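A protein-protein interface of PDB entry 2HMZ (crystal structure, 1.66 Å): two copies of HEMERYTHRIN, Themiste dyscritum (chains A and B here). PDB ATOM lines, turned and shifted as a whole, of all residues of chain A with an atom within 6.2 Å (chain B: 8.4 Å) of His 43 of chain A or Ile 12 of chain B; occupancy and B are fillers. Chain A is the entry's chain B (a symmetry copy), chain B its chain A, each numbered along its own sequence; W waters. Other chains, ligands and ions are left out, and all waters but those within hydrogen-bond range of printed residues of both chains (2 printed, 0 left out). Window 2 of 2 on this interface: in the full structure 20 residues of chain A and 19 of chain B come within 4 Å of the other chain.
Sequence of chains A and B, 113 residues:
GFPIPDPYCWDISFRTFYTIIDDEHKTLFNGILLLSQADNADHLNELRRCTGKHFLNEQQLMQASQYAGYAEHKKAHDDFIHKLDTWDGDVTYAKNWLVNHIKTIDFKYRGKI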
ATOM      1  N   GLY A  31       6.869 -20.042   6.605  1.00  0.00           N
ATOM      2  CA  GLY A  31       7.271 -20.777   7.793  1.00  0.00           C
ATOM      3  C   GLY A  31       6.050 -21.018   8.722  1.00  0.00           C
ATOM      4  O   GLY A  31       5.898 -22.164   9.189  1.00  0.00           O
ATOM      5  N   LEU A  33       2.868 -20.822   7.764  1.00  0.00           N
ATOM      6  CA  LEU A  33       1.986 -21.691   7.031  1.00  0.00           C
ATOM      7  C   LEU A  33       2.380 -23.161   7.301  1.00  0.00           C
ATOM      8  O   LEU A  33       1.453 -23.939   7.639  1.00  0.00           O
ATOM      9  CB  LEU A  33       1.935 -21.409   5.528  1.00  0.00           C
ATOM     10  CG  LEU A  33       0.923 -22.311   4.795  1.00  0.00           C
ATOM     11  CD1 LEU A  33      -0.509 -21.867   5.055  1.00  0.00           C
ATOM     12  CD2 LEU A  33       1.151 -22.308   3.321  1.00  0.00           C
ATOM     13  N   LEU A  34       3.603 -23.563   7.175  1.00  0.00           N
ATOM     14  CA  LEU A  34       4.023 -24.932   7.454  1.00  0.00           C
ATOM     15  C   LEU A  34       3.604 -25.390   8.845  1.00  0.00           C
ATOM     16  O   LEU A  34       3.164 -26.548   8.943  1.00  0.00           O
ATOM     17  CB  LEU A  34       5.524 -25.104   7.294  1.00  0.00           C
ATOM     18  CG  LEU A  34       6.045 -24.744   5.875  1.00  0.00           C
ATOM     19  CD1 LEU A  34       7.554 -24.913   5.881  1.00  0.00           C
ATOM     20  CD2 LEU A  34       5.309 -25.549   4.854  1.00  0.00           C
ATOM     21  N   LEU A  35       3.835 -24.630   9.833  1.00  0.00           N
ATOM     22  CA  LEU A  35       3.504 -24.948  11.210  1.00  0.00           C
ATOM     23  C   LEU A  35       1.992 -25.143  11.341  1.00  0.00           C
ATOM     24  O   LEU A  35       1.537 -26.014  12.051  1.00  0.00           O
ATOM     25  CB  LEU A  35       3.993 -23.876  12.142  1.00  0.00           C
ATOM     26  CG  LEU A  35       5.452 -23.978  12.531  1.00  0.00           C
ATOM     27  CD1 LEU A  35       5.679 -22.728  13.415  1.00  0.00           C
ATOM     28  CD2 LEU A  35       5.807 -25.213  13.294  1.00  0.00           C
ATOM     29  N   SER A  36       1.294 -24.322  10.612  1.00  0.00           N
ATOM     30  CA  SER A  36      -0.186 -24.396  10.627  1.00  0.00           C
ATOM     31  C   SER A  36      -0.581 -25.734  10.034  1.00  0.00           C
ATOM     32  O   SER A  36      -1.694 -26.228  10.302  1.00  0.00           O
ATOM     33  CB  SER A  36      -0.779 -23.203   9.952  1.00  0.00           C
ATOM     34  OG  SER A  36      -1.216 -23.301   8.653  1.00  0.00           O
ATOM     35  N   GLN A  37       0.212 -26.330   9.191  1.00  0.00           N
ATOM     36  CA  GLN A  37      -0.100 -27.614   8.560  1.00  0.00           C
ATOM     37  C   GLN A  37       0.392 -28.788   9.381  1.00  0.00           C
ATOM     38  O   GLN A  37      -0.351 -29.810   9.471  1.00  0.00           O
ATOM     39  CB  GLN A  37       0.435 -27.700   7.130  1.00  0.00           C
ATOM     40  CG  GLN A  37      -0.193 -26.570   6.303  1.00  0.00           C
ATOM     41  CD  GLN A  37       0.273 -26.512   4.870  1.00  0.00           C
ATOM     42  OE1 GLN A  37      -0.547 -26.256   3.957  1.00  0.00           O
ATOM     43  NE2 GLN A  37       1.583 -26.692   4.669  1.00  0.00           N
ATOM     44  N   ALA A  38       1.536 -28.736   9.986  1.00  0.00           N
ATOM     45  CA  ALA A  38       2.076 -29.842  10.739  1.00  0.00           C
ATOM     46  C   ALA A  38       3.004 -29.183  11.753  1.00  0.00           C
ATOM     47  O   ALA A  38       3.954 -28.592  11.313  1.00  0.00           O
ATOM     48  CB  ALA A  38       2.872 -30.849   9.915  1.00  0.00           C
ATOM     49  N   ASP A  39       2.621 -29.280  12.987  1.00  0.00           N
ATOM     50  CA  ASP A  39       3.496 -28.677  14.017  1.00  0.00           C
ATOM     51  C   ASP A  39       4.553 -29.707  14.335  1.00  0.00           C
ATOM     52  O   ASP A  39       4.431 -30.510  15.266  1.00  0.00           O
ATOM     53  CB  ASP A  39       2.668 -28.166  15.170  1.00  0.00           C
ATOM     54  CG  ASP A  39       3.430 -27.509  16.301  1.00  0.00           C
ATOM     55  OD1 ASP A  39       2.802 -27.046  17.302  1.00  0.00           O
ATOM     56  OD2 ASP A  39       4.682 -27.463  16.225  1.00  0.00           O
ATOM     57  N   ASN A  40       5.641 -29.598  13.618  1.00  0.00           N
ATOM     58  CA  ASN A  40       6.766 -30.539  13.857  1.00  0.00           C
ATOM     59  C   ASN A  40       8.070 -29.740  13.917  1.00  0.00           C
ATOM     60  O   ASN A  40       8.131 -28.538  13.587  1.00  0.00           O
ATOM     61  CB  ASN A  40       6.672 -31.645  12.816  1.00  0.00           C
ATOM     62  CG  ASN A  40       6.908 -31.294  11.380  1.00  0.00           C
ATOM     63  OD1 ASN A  40       6.351 -31.935  10.440  1.00  0.00           O
ATOM     64  ND2 ASN A  40       7.722 -30.275  11.117  1.00  0.00           N
ATOM     65  N   ALA A  41       9.158 -30.443  14.106  1.00  0.00           N
ATOM     66  CA  ALA A  41      10.501 -29.857  14.151  1.00  0.00           C
ATOM     67  C   ALA A  41      10.997 -29.423  12.774  1.00  0.00           C
ATOM     68  O   ALA A  41      11.698 -28.354  12.759  1.00  0.00           O
ATOM     69  CB  ALA A  41      11.499 -30.798  14.827  1.00  0.00           C
ATOM     70  N   ASP A  42      10.784 -30.103  11.671  1.00  0.00           N
ATOM     71  CA  ASP A  42      11.241 -29.573  10.408  1.00  0.00           C
ATOM     72  C   ASP A  42      10.692 -28.181  10.156  1.00  0.00           C
ATOM     73  O   ASP A  42      11.373 -27.313   9.651  1.00  0.00           O
ATOM     74  CB  ASP A  42      10.779 -30.487   9.250  1.00  0.00           C
ATOM     75  CG  ASP A  42      11.884 -31.527   9.143  1.00  0.00           C
ATOM     76  OD1 ASP A  42      13.050 -31.137   9.029  1.00  0.00           O
ATOM     77  OD2 ASP A  42      11.572 -32.668   9.487  1.00  0.00           O
ATOM     78  N   HIS A  43       9.398 -28.106  10.356  1.00  0.00           N
ATOM     79  CA  HIS A  43       8.718 -26.807  10.107  1.00  0.00           C
ATOM     80  C   HIS A  43       9.151 -25.711  10.997  1.00  0.00           C
ATOM     81  O   HIS A  43       9.236 -24.519  10.613  1.00  0.00           O
ATOM     82  CB  HIS A  43       7.188 -27.037  10.172  1.00  0.00           C
ATOM     83  CG  HIS A  43       6.763 -27.927   9.035  1.00  0.00           C
ATOM     84  ND1 HIS A  43       5.470 -28.397   8.944  1.00  0.00           N
ATOM     85  CD2 HIS A  43       7.379 -28.396   7.924  1.00  0.00           C
ATOM     86  CE1 HIS A  43       5.322 -29.038   7.799  1.00  0.00           C
ATOM     87  NE2 HIS A  43       6.456 -29.067   7.174  1.00  0.00           N
ATOM     88  N   LEU A  44       9.357 -26.020  12.269  1.00  0.00           N
ATOM     89  CA  LEU A  44       9.831 -25.020  13.215  1.00  0.00           C
ATOM     90  C   LEU A  44      11.275 -24.619  12.908  1.00  0.00           C
ATOM     91  O   LEU A  44      11.571 -23.420  13.073  1.00  0.00           O
ATOM     92  CB  LEU A  44       9.599 -25.521  14.645  1.00  0.00           C
ATOM     93  CG  LEU A  44      10.071 -24.540  15.737  1.00  0.00           C
ATOM     94  CD1 LEU A  44       9.159 -23.327  15.786  1.00  0.00           C
ATOM     95  CD2 LEU A  44      10.107 -25.336  17.062  1.00  0.00           C
ATOM     96  N   ASN A  45      12.140 -25.498  12.504  1.00  0.00           N
ATOM     97  CA  ASN A  45      13.553 -25.179  12.197  1.00  0.00           C
ATOM     98  C   ASN A  45      13.637 -24.174  11.032  1.00  0.00           C
ATOM     99  O   ASN A  45      14.425 -23.283  10.976  1.00  0.00           O
ATOM    100  CB  ASN A  45      14.271 -26.451  11.795  1.00  0.00           C
ATOM    101  CG  ASN A  45      14.592 -27.340  12.999  1.00  0.00           C
ATOM    102  OD1 ASN A  45      14.918 -28.539  12.729  1.00  0.00           O
ATOM    103  ND2 ASN A  45      14.526 -26.888  14.223  1.00  0.00           N
ATOM    104  N   GLU A  46      12.755 -24.523  10.065  1.00  0.00           N
ATOM    105  CA  GLU A  46      12.621 -23.708   8.848  1.00  0.00           C
ATOM    106  C   GLU A  46      12.216 -22.295   9.211  1.00  0.00           C
ATOM    107  O   GLU A  46      12.914 -21.316   8.817  1.00  0.00           O
ATOM    108  CB  GLU A  46      11.605 -24.272   7.856  1.00  0.00           C
ATOM    109  CG  GLU A  46      11.760 -23.812   6.415  1.00  0.00           C
ATOM    110  CD  GLU A  46      13.066 -24.136   5.726  1.00  0.00           C
ATOM    111  OE1 GLU A  46      13.504 -23.516   4.785  1.00  0.00           O
ATOM    112  OE2 GLU A  46      13.600 -25.221   6.104  1.00  0.00           O
ATOM    113  N   LEU A  47      11.101 -22.159  10.003  1.00  0.00           N
ATOM    114  CA  LEU A  47      10.667 -20.814  10.403  1.00  0.00           C
ATOM    115  C   LEU A  47      11.769 -20.179  11.265  1.00  0.00           C
ATOM    116  O   LEU A  47      12.047 -18.987  11.086  1.00  0.00           O
ATOM    117  CB  LEU A  47       9.300 -20.867  11.098  1.00  0.00           C
ATOM    118  CG  LEU A  47       8.863 -19.567  11.759  1.00  0.00           C
ATOM    119  CD1 LEU A  47       8.516 -18.520  10.656  1.00  0.00           C
ATOM    120  CD2 LEU A  47       7.679 -19.769  12.661  1.00  0.00           C
ATOM    121  N   ARG A  48      12.362 -20.871  12.216  1.00  0.00           N
ATOM    122  CA  ARG A  48      13.349 -20.330  13.107  1.00  0.00           C
ATOM    123  C   ARG A  48      14.584 -19.813  12.370  1.00  0.00           C
ATOM    124  O   ARG A  48      15.045 -18.720  12.721  1.00  0.00           O
ATOM    125  CB  ARG A  48      13.721 -21.352  14.193  1.00  0.00           C
ATOM    126  CG  ARG A  48      14.800 -20.870  15.102  1.00  0.00           C
ATOM    127  CD  ARG A  48      14.366 -19.647  15.893  1.00  0.00           C
ATOM    128  NE  ARG A  48      15.326 -19.290  16.879  1.00  0.00           N
ATOM    129  CZ  ARG A  48      16.534 -18.711  16.780  1.00  0.00           C
ATOM    130  NH1 ARG A  48      17.214 -18.493  17.898  1.00  0.00           N
ATOM    131  NH2 ARG A  48      16.988 -18.301  15.589  1.00  0.00           N
ATOM    132  N   CYS B   9       1.897 -23.187  -2.096  1.00  0.00           N
ATOM    133  CA  CYS B   9       3.027 -22.674  -1.361  1.00  0.00           C
ATOM    134  C   CYS B   9       4.034 -23.865  -1.219  1.00  0.00           C
ATOM    135  O   CYS B   9       3.776 -25.050  -1.461  1.00  0.00           O
ATOM    136  CB  CYS B   9       2.728 -22.055  -0.030  1.00  0.00           C
ATOM    137  SG  CYS B   9       1.780 -20.531  -0.033  1.00  0.00           S
ATOM    138  N   TRP B  10       5.249 -23.328  -0.993  1.00  0.00           N
ATOM    139  CA  TRP B  10       6.414 -24.225  -0.850  1.00  0.00           C
ATOM    140  C   TRP B  10       6.204 -25.156   0.318  1.00  0.00           C
ATOM    141  O   TRP B  10       5.640 -24.705   1.367  1.00  0.00           O
ATOM    142  CB  TRP B  10       7.665 -23.300  -0.714  1.00  0.00           C
ATOM    143  CG  TRP B  10       8.996 -23.982  -0.670  1.00  0.00           C
ATOM    144  CD1 TRP B  10       9.888 -24.168  -1.729  1.00  0.00           C
ATOM    145  CD2 TRP B  10       9.617 -24.479   0.506  1.00  0.00           C
ATOM    146  NE1 TRP B  10      11.020 -24.763  -1.251  1.00  0.00           N
ATOM    147  CE2 TRP B  10      10.911 -24.972   0.084  1.00  0.00           C
ATOM    148  CE3 TRP B  10       9.243 -24.594   1.832  1.00  0.00           C
ATOM    149  CZ2 TRP B  10      11.758 -25.546   1.039  1.00  0.00           C
ATOM    150  CZ3 TRP B  10      10.066 -25.140   2.775  1.00  0.00           C
ATOM    151  CH2 TRP B  10      11.359 -25.593   2.368  1.00  0.00           C
ATOM    152  N   ASP B  11       6.680 -26.368   0.210  1.00  0.00           N
ATOM    153  CA  ASP B  11       6.685 -27.288   1.404  1.00  0.00           C
ATOM    154  C   ASP B  11       8.076 -27.910   1.432  1.00  0.00           C
ATOM    155  O   ASP B  11       8.822 -27.834   0.405  1.00  0.00           O
ATOM    156  CB  ASP B  11       5.504 -28.202   1.347  1.00  0.00           C
ATOM    157  CG  ASP B  11       5.543 -29.232   0.227  1.00  0.00           C
ATOM    158  OD1 ASP B  11       6.494 -30.002   0.087  1.00  0.00           O
ATOM    159  OD2 ASP B  11       4.600 -29.280  -0.598  1.00  0.00           O
ATOM    160  N   ILE B  12       8.402 -28.616   2.513  1.00  0.00           N
ATOM    161  CA  ILE B  12       9.753 -29.173   2.662  1.00  0.00           C
ATOM    162  C   ILE B  12      10.104 -30.297   1.708  1.00  0.00           C
ATOM    163  O   ILE B  12      11.291 -30.667   1.569  1.00  0.00           O
ATOM    164  CB  ILE B  12      10.084 -29.566   4.168  1.00  0.00           C
ATOM    165  CG1 ILE B  12       9.171 -30.727   4.520  1.00  0.00           C
ATOM    166  CG2 ILE B  12      10.031 -28.349   5.118  1.00  0.00           C
ATOM    167  CD1 ILE B  12       9.474 -31.526   5.782  1.00  0.00           C
ATOM    168  N   SER B  13       9.140 -30.803   0.944  1.00  0.00           N
ATOM    169  CA  SER B  13       9.437 -31.825  -0.052  1.00  0.00           C
ATOM    170  C   SER B  13      10.292 -31.208  -1.191  1.00  0.00           C
ATOM    171  O   SER B  13      10.873 -31.968  -1.953  1.00  0.00           O
ATOM    172  CB  SER B  13       8.188 -32.501  -0.597  1.00  0.00           C
ATOM    173  OG  SER B  13       7.411 -31.791  -1.518  1.00  0.00           O
ATOM    174  N   PHE B  14      10.242 -29.870  -1.304  1.00  0.00           N
ATOM    175  CA  PHE B  14      10.965 -29.134  -2.367  1.00  0.00           C
ATOM    176  C   PHE B  14      12.354 -28.778  -1.907  1.00  0.00           C
ATOM    177  O   PHE B  14      13.069 -28.137  -2.658  1.00  0.00           O
ATOM    178  CB  PHE B  14      10.166 -27.855  -2.742  1.00  0.00           C
ATOM    179  CG  PHE B  14       8.979 -28.215  -3.585  1.00  0.00           C
ATOM    180  CD1 PHE B  14       7.745 -28.439  -2.897  1.00  0.00           C
ATOM    181  CD2 PHE B  14       9.049 -28.364  -4.945  1.00  0.00           C
ATOM    182  CE1 PHE B  14       6.630 -28.826  -3.634  1.00  0.00           C
ATOM    183  CE2 PHE B  14       7.948 -28.752  -5.729  1.00  0.00           C
ATOM    184  CZ  PHE B  14       6.718 -28.966  -5.040  1.00  0.00           C
ATOM    185  N   ARG B  15      12.719 -29.169  -0.698  1.00  0.00           N
ATOM    186  CA  ARG B  15      14.028 -28.815  -0.184  1.00  0.00           C
ATOM    187  C   ARG B  15      15.170 -29.266  -1.061  1.00  0.00           C
ATOM    188  O   ARG B  15      15.236 -30.418  -1.452  1.00  0.00           O
ATOM    189  CB  ARG B  15      14.294 -29.416   1.180  1.00  0.00           C
ATOM    190  CG  ARG B  15      13.997 -28.495   2.309  1.00  0.00           C
ATOM    191  CD  ARG B  15      14.365 -29.197   3.588  1.00  0.00           C
ATOM    192  NE  ARG B  15      13.812 -28.413   4.682  1.00  0.00           N
ATOM    193  CZ  ARG B  15      13.519 -28.922   5.892  1.00  0.00           C
ATOM    194  NH1 ARG B  15      13.647 -30.260   6.068  1.00  0.00           N
ATOM    195  NH2 ARG B  15      13.380 -28.063   6.968  1.00  0.00           N
ATOM    196  N   THR B  16      16.117 -28.328  -1.311  1.00  0.00           N
ATOM    197  CA  THR B  16      17.287 -28.651  -2.077  1.00  0.00           C
ATOM    198  C   THR B  16      18.488 -28.797  -1.162  1.00  0.00           C
ATOM    199  O   THR B  16      19.531 -29.318  -1.593  1.00  0.00           O
ATOM    200  CB  THR B  16      17.615 -27.583  -3.229  1.00  0.00           C
ATOM    201  OG1 THR B  16      18.031 -26.414  -2.454  1.00  0.00           O
ATOM    202  CG2 THR B  16      16.509 -27.391  -4.233  1.00  0.00           C
ATOM    203  N   PHE B  17      18.407 -28.307   0.064  1.00  0.00           N
ATOM    204  CA  PHE B  17      19.562 -28.325   1.019  1.00  0.00           C
ATOM    205  C   PHE B  17      20.508 -27.176   0.864  1.00  0.00           C
ATOM    206  O   PHE B  17      21.451 -26.905   1.665  1.00  0.00           O
ATOM    207  CB  PHE B  17      20.260 -29.724   1.021  1.00  0.00           C
ATOM    208  CG  PHE B  17      19.173 -30.708   1.476  1.00  0.00           C
ATOM    209  CD1 PHE B  17      18.567 -30.583   2.735  1.00  0.00           C
ATOM    210  CD2 PHE B  17      18.671 -31.611   0.543  1.00  0.00           C
ATOM    211  CE1 PHE B  17      17.535 -31.401   3.136  1.00  0.00           C
ATOM    212  CE2 PHE B  17      17.583 -32.448   0.915  1.00  0.00           C
ATOM    213  CZ  PHE B  17      17.016 -32.324   2.206  1.00  0.00           C
ATOM    214  N   ASP B  22      16.513 -22.531  -1.463  1.00  0.00           N
ATOM    215  CA  ASP B  22      15.180 -22.796  -0.912  1.00  0.00           C
ATOM    216  C   ASP B  22      14.440 -21.502  -0.631  1.00  0.00           C
ATOM    217  O   ASP B  22      13.238 -21.470  -0.899  1.00  0.00           O
ATOM    218  CB  ASP B  22      15.221 -23.675   0.368  1.00  0.00           C
ATOM    219  CG  ASP B  22      15.709 -25.086  -0.004  1.00  0.00           C
ATOM    220  OD1 ASP B  22      15.641 -25.525  -1.158  1.00  0.00           O
ATOM    221  OD2 ASP B  22      16.141 -25.745   0.959  1.00  0.00           O
ATOM    222  N   LYS B  26      10.766 -20.278  -2.403  1.00  0.00           N
ATOM    223  CA  LYS B  26       9.535 -19.871  -1.665  1.00  0.00           C
ATOM    224  C   LYS B  26       8.932 -18.678  -2.339  1.00  0.00           C
ATOM    225  O   LYS B  26       7.733 -18.538  -2.451  1.00  0.00           O
ATOM    226  CB  LYS B  26       9.914 -19.618  -0.215  1.00  0.00           C
ATOM    227  CG  LYS B  26      10.266 -20.877   0.574  1.00  0.00           C
ATOM    228  CD  LYS B  26      10.822 -20.570   1.944  1.00  0.00           C
ATOM    229  CE  LYS B  26      11.579 -21.757   2.513  1.00  0.00           C
ATOM    230  NZ  LYS B  26      12.290 -21.401   3.747  1.00  0.00           N
ATOM    231  N   LYS B 103      11.639 -30.180  -8.800  1.00  0.00           N
ATOM    232  CA  LYS B 103      11.814 -31.620  -8.438  1.00  0.00           C
ATOM    233  C   LYS B 103      12.502 -32.420  -9.484  1.00  0.00           C
ATOM    234  O   LYS B 103      13.085 -33.493  -9.191  1.00  0.00           O
ATOM    235  CB  LYS B 103      10.451 -32.187  -8.024  1.00  0.00           C
ATOM    236  CG  LYS B 103      10.094 -31.723  -6.628  1.00  0.00           C
ATOM    237  CD  LYS B 103       8.814 -32.331  -6.152  1.00  0.00           C
ATOM    238  CE  LYS B 103       8.659 -32.227  -4.661  1.00  0.00           C
ATOM    239  NZ  LYS B 103       7.316 -32.674  -4.219  1.00  0.00           N
ATOM    240  N   PHE B 107      16.717 -30.421  -8.702  1.00  0.00           N
ATOM    241  CA  PHE B 107      17.219 -31.520  -7.831  1.00  0.00           C
ATOM    242  C   PHE B 107      18.463 -32.189  -8.402  1.00  0.00           C
ATOM    243  O   PHE B 107      19.195 -32.808  -7.615  1.00  0.00           O
ATOM    244  CB  PHE B 107      16.110 -32.541  -7.538  1.00  0.00           C
ATOM    245  CG  PHE B 107      15.191 -32.193  -6.421  1.00  0.00           C
ATOM    246  CD1 PHE B 107      14.447 -33.234  -5.814  1.00  0.00           C
ATOM    247  CD2 PHE B 107      15.070 -30.887  -5.869  1.00  0.00           C
ATOM    248  CE1 PHE B 107      13.559 -32.931  -4.804  1.00  0.00           C
ATOM    249  CE2 PHE B 107      14.259 -30.623  -4.807  1.00  0.00           C
ATOM    250  CZ  PHE B 107      13.452 -31.657  -4.273  1.00  0.00           C
ATOM    251  N   ARG B 110      21.970 -31.023  -6.928  1.00  0.00           N
ATOM    252  CA  ARG B 110      22.292 -31.312  -5.501  1.00  0.00           C
ATOM    253  C   ARG B 110      23.532 -32.217  -5.326  1.00  0.00           C
ATOM    254  O   ARG B 110      23.721 -33.236  -6.015  1.00  0.00           O
ATOM    255  CB  ARG B 110      21.074 -31.945  -4.791  1.00  0.00           C
ATOM    256  CG  ARG B 110      19.818 -31.030  -4.956  1.00  0.00           C
ATOM    257  CD  ARG B 110      18.763 -31.507  -3.948  1.00  0.00           C
ATOM    258  NE  ARG B 110      18.292 -32.784  -4.386  1.00  0.00           N
ATOM    259  CZ  ARG B 110      17.371 -33.544  -3.793  1.00  0.00           C
ATOM    260  NH1 ARG B 110      16.683 -33.260  -2.711  1.00  0.00           N
ATOM    261  NH2 ARG B 110      17.192 -34.686  -4.480  1.00  0.00           N
HETATM  262  O   HOH W   1       9.861 -20.741   5.245  1.00  0.00           O
HETATM  263  O   HOH W   2      15.455 -25.403   3.649  1.00  0.00           O
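The side-chain carboxylate (OD1) of Asp 42 of chain A is in salt-bridge range of the guanidinium group (NH1) of Arg 15 of chain B, 3.1 Å away. NH2 of Arg 15 of chain B is in salt-bridge range of OE2 of Glu 46 of chain A (3.0 Å). The side-chain amino group (NZ) of Lys 26 of chain B lies within salt-bridge range of the side-chain carboxylate (OE1) of Glu 46 of chain A (2.7 Å).
The backbone carbonyl oxygen of Arg 15 of chain B is in hydrogen-bond range of the guanidinium group of Arg 110 of chain B. The backbone carbonyl oxygen of Leu 33 of chain A lies within hydrogen-bond range of the side-chain hydroxyl of Ser 36 of chain A, 2.9 Å away. The backbone carbonyl oxygen of Leu 34 of chain A lies within hydrogen-bond range of a ring nitrogen (ND1) of His 43 of chain A (3.0 Å). O of Ala 38 of chain A is in hydrogen-bond range of ND1 of His 43 of chain A (2.8 Å). ND2 of Asn 40 of chain A sits close to N of Asp 42 of chain A (3.1 Å). N of His 43 of chain A sits close to ND2 of Asn 40 of chain A, at 2.8 Å.
Cys 9 of chain B touches Leu 33 of chain A (CB to CD2, 3.7 Å). Leu 34 of chain A touches Trp 10 of chain B. CB of Asp 42 of chain A touches CD1 of Ile 12 of chain B (3.8 Å). His 43 of chain A touches Ile 12 of chain B (CD2 to CG2, 3.9 Å). OE1 of Glu 46 of chain A touches CH2 of Trp 10 of chain B (3.8 Å).
No residue of chain B comes within 4 Å of Ala 38 of chain A. Of the printed residues of chain B, Asp 42 of chain A touches Ile 12 (3.8 Å) and Arg 15 (3.1 Å). Printed residues of chain B within 4 Å of His 43 of chain A: Ile 12. Of the printed residues of chain B, Glu 46 of chain A touches Trp 10 (3.8 Å), Arg 15 (3.0 Å) and Lys 26 (2.7 Å). Arg 48 of chain A touches none of the printed residues of chain B. Of the printed residues of chain A, Cys 9 of chain B touches Leu 33. Asp 11 of chain B touches none of the printed residues of chain A. Ile 12 of chain B touches two residues of chain A. Of the printed residues of chain A, Arg 15 of chain B touches Asp 42 and Glu 46. Printed residues of chain A within 4 Å of Lys 26 of chain B: Glu 46. The nearest printed residue of chain B that does not touch Leu 34 of chain A is Asp 11 of chain B (4.1 Å).
Hydrophobic or aromatic side chains of chain A that line the printed part of chain B: Leu 33, Leu 34 and His 43. Printed residues of chain B that touch a printed residue of chain A: Cys 9, Trp 10, Ile 12, Arg 15 and Lys 26. Hydrophobic or aromatic side chains of chain B that line the printed part of chain A: Trp 10 and Ile 12. Among the printed residues, Asp or Glu carboxylates within 4 Å of a Lys or Arg side-chain nitrogen of the other chain: Asp 42 of chain A with Arg 15 of chain B (3.1 Å), Glu 46 of chain A with Arg 15 of chain B (3.0 Å) and Glu 46 of chain A with Lys 26 of chain B (2.7 Å).
No position is printed for both chains.
Water W2 lies within hydrogen-bond range of OD2 of Asp 22 of chain B and OE1 of Glu 46 of chain A. Water W1 bridges NZ of Lys 26 of chain B (2.9 Å) and N of Gly 31 of chain A (3.4 Å).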
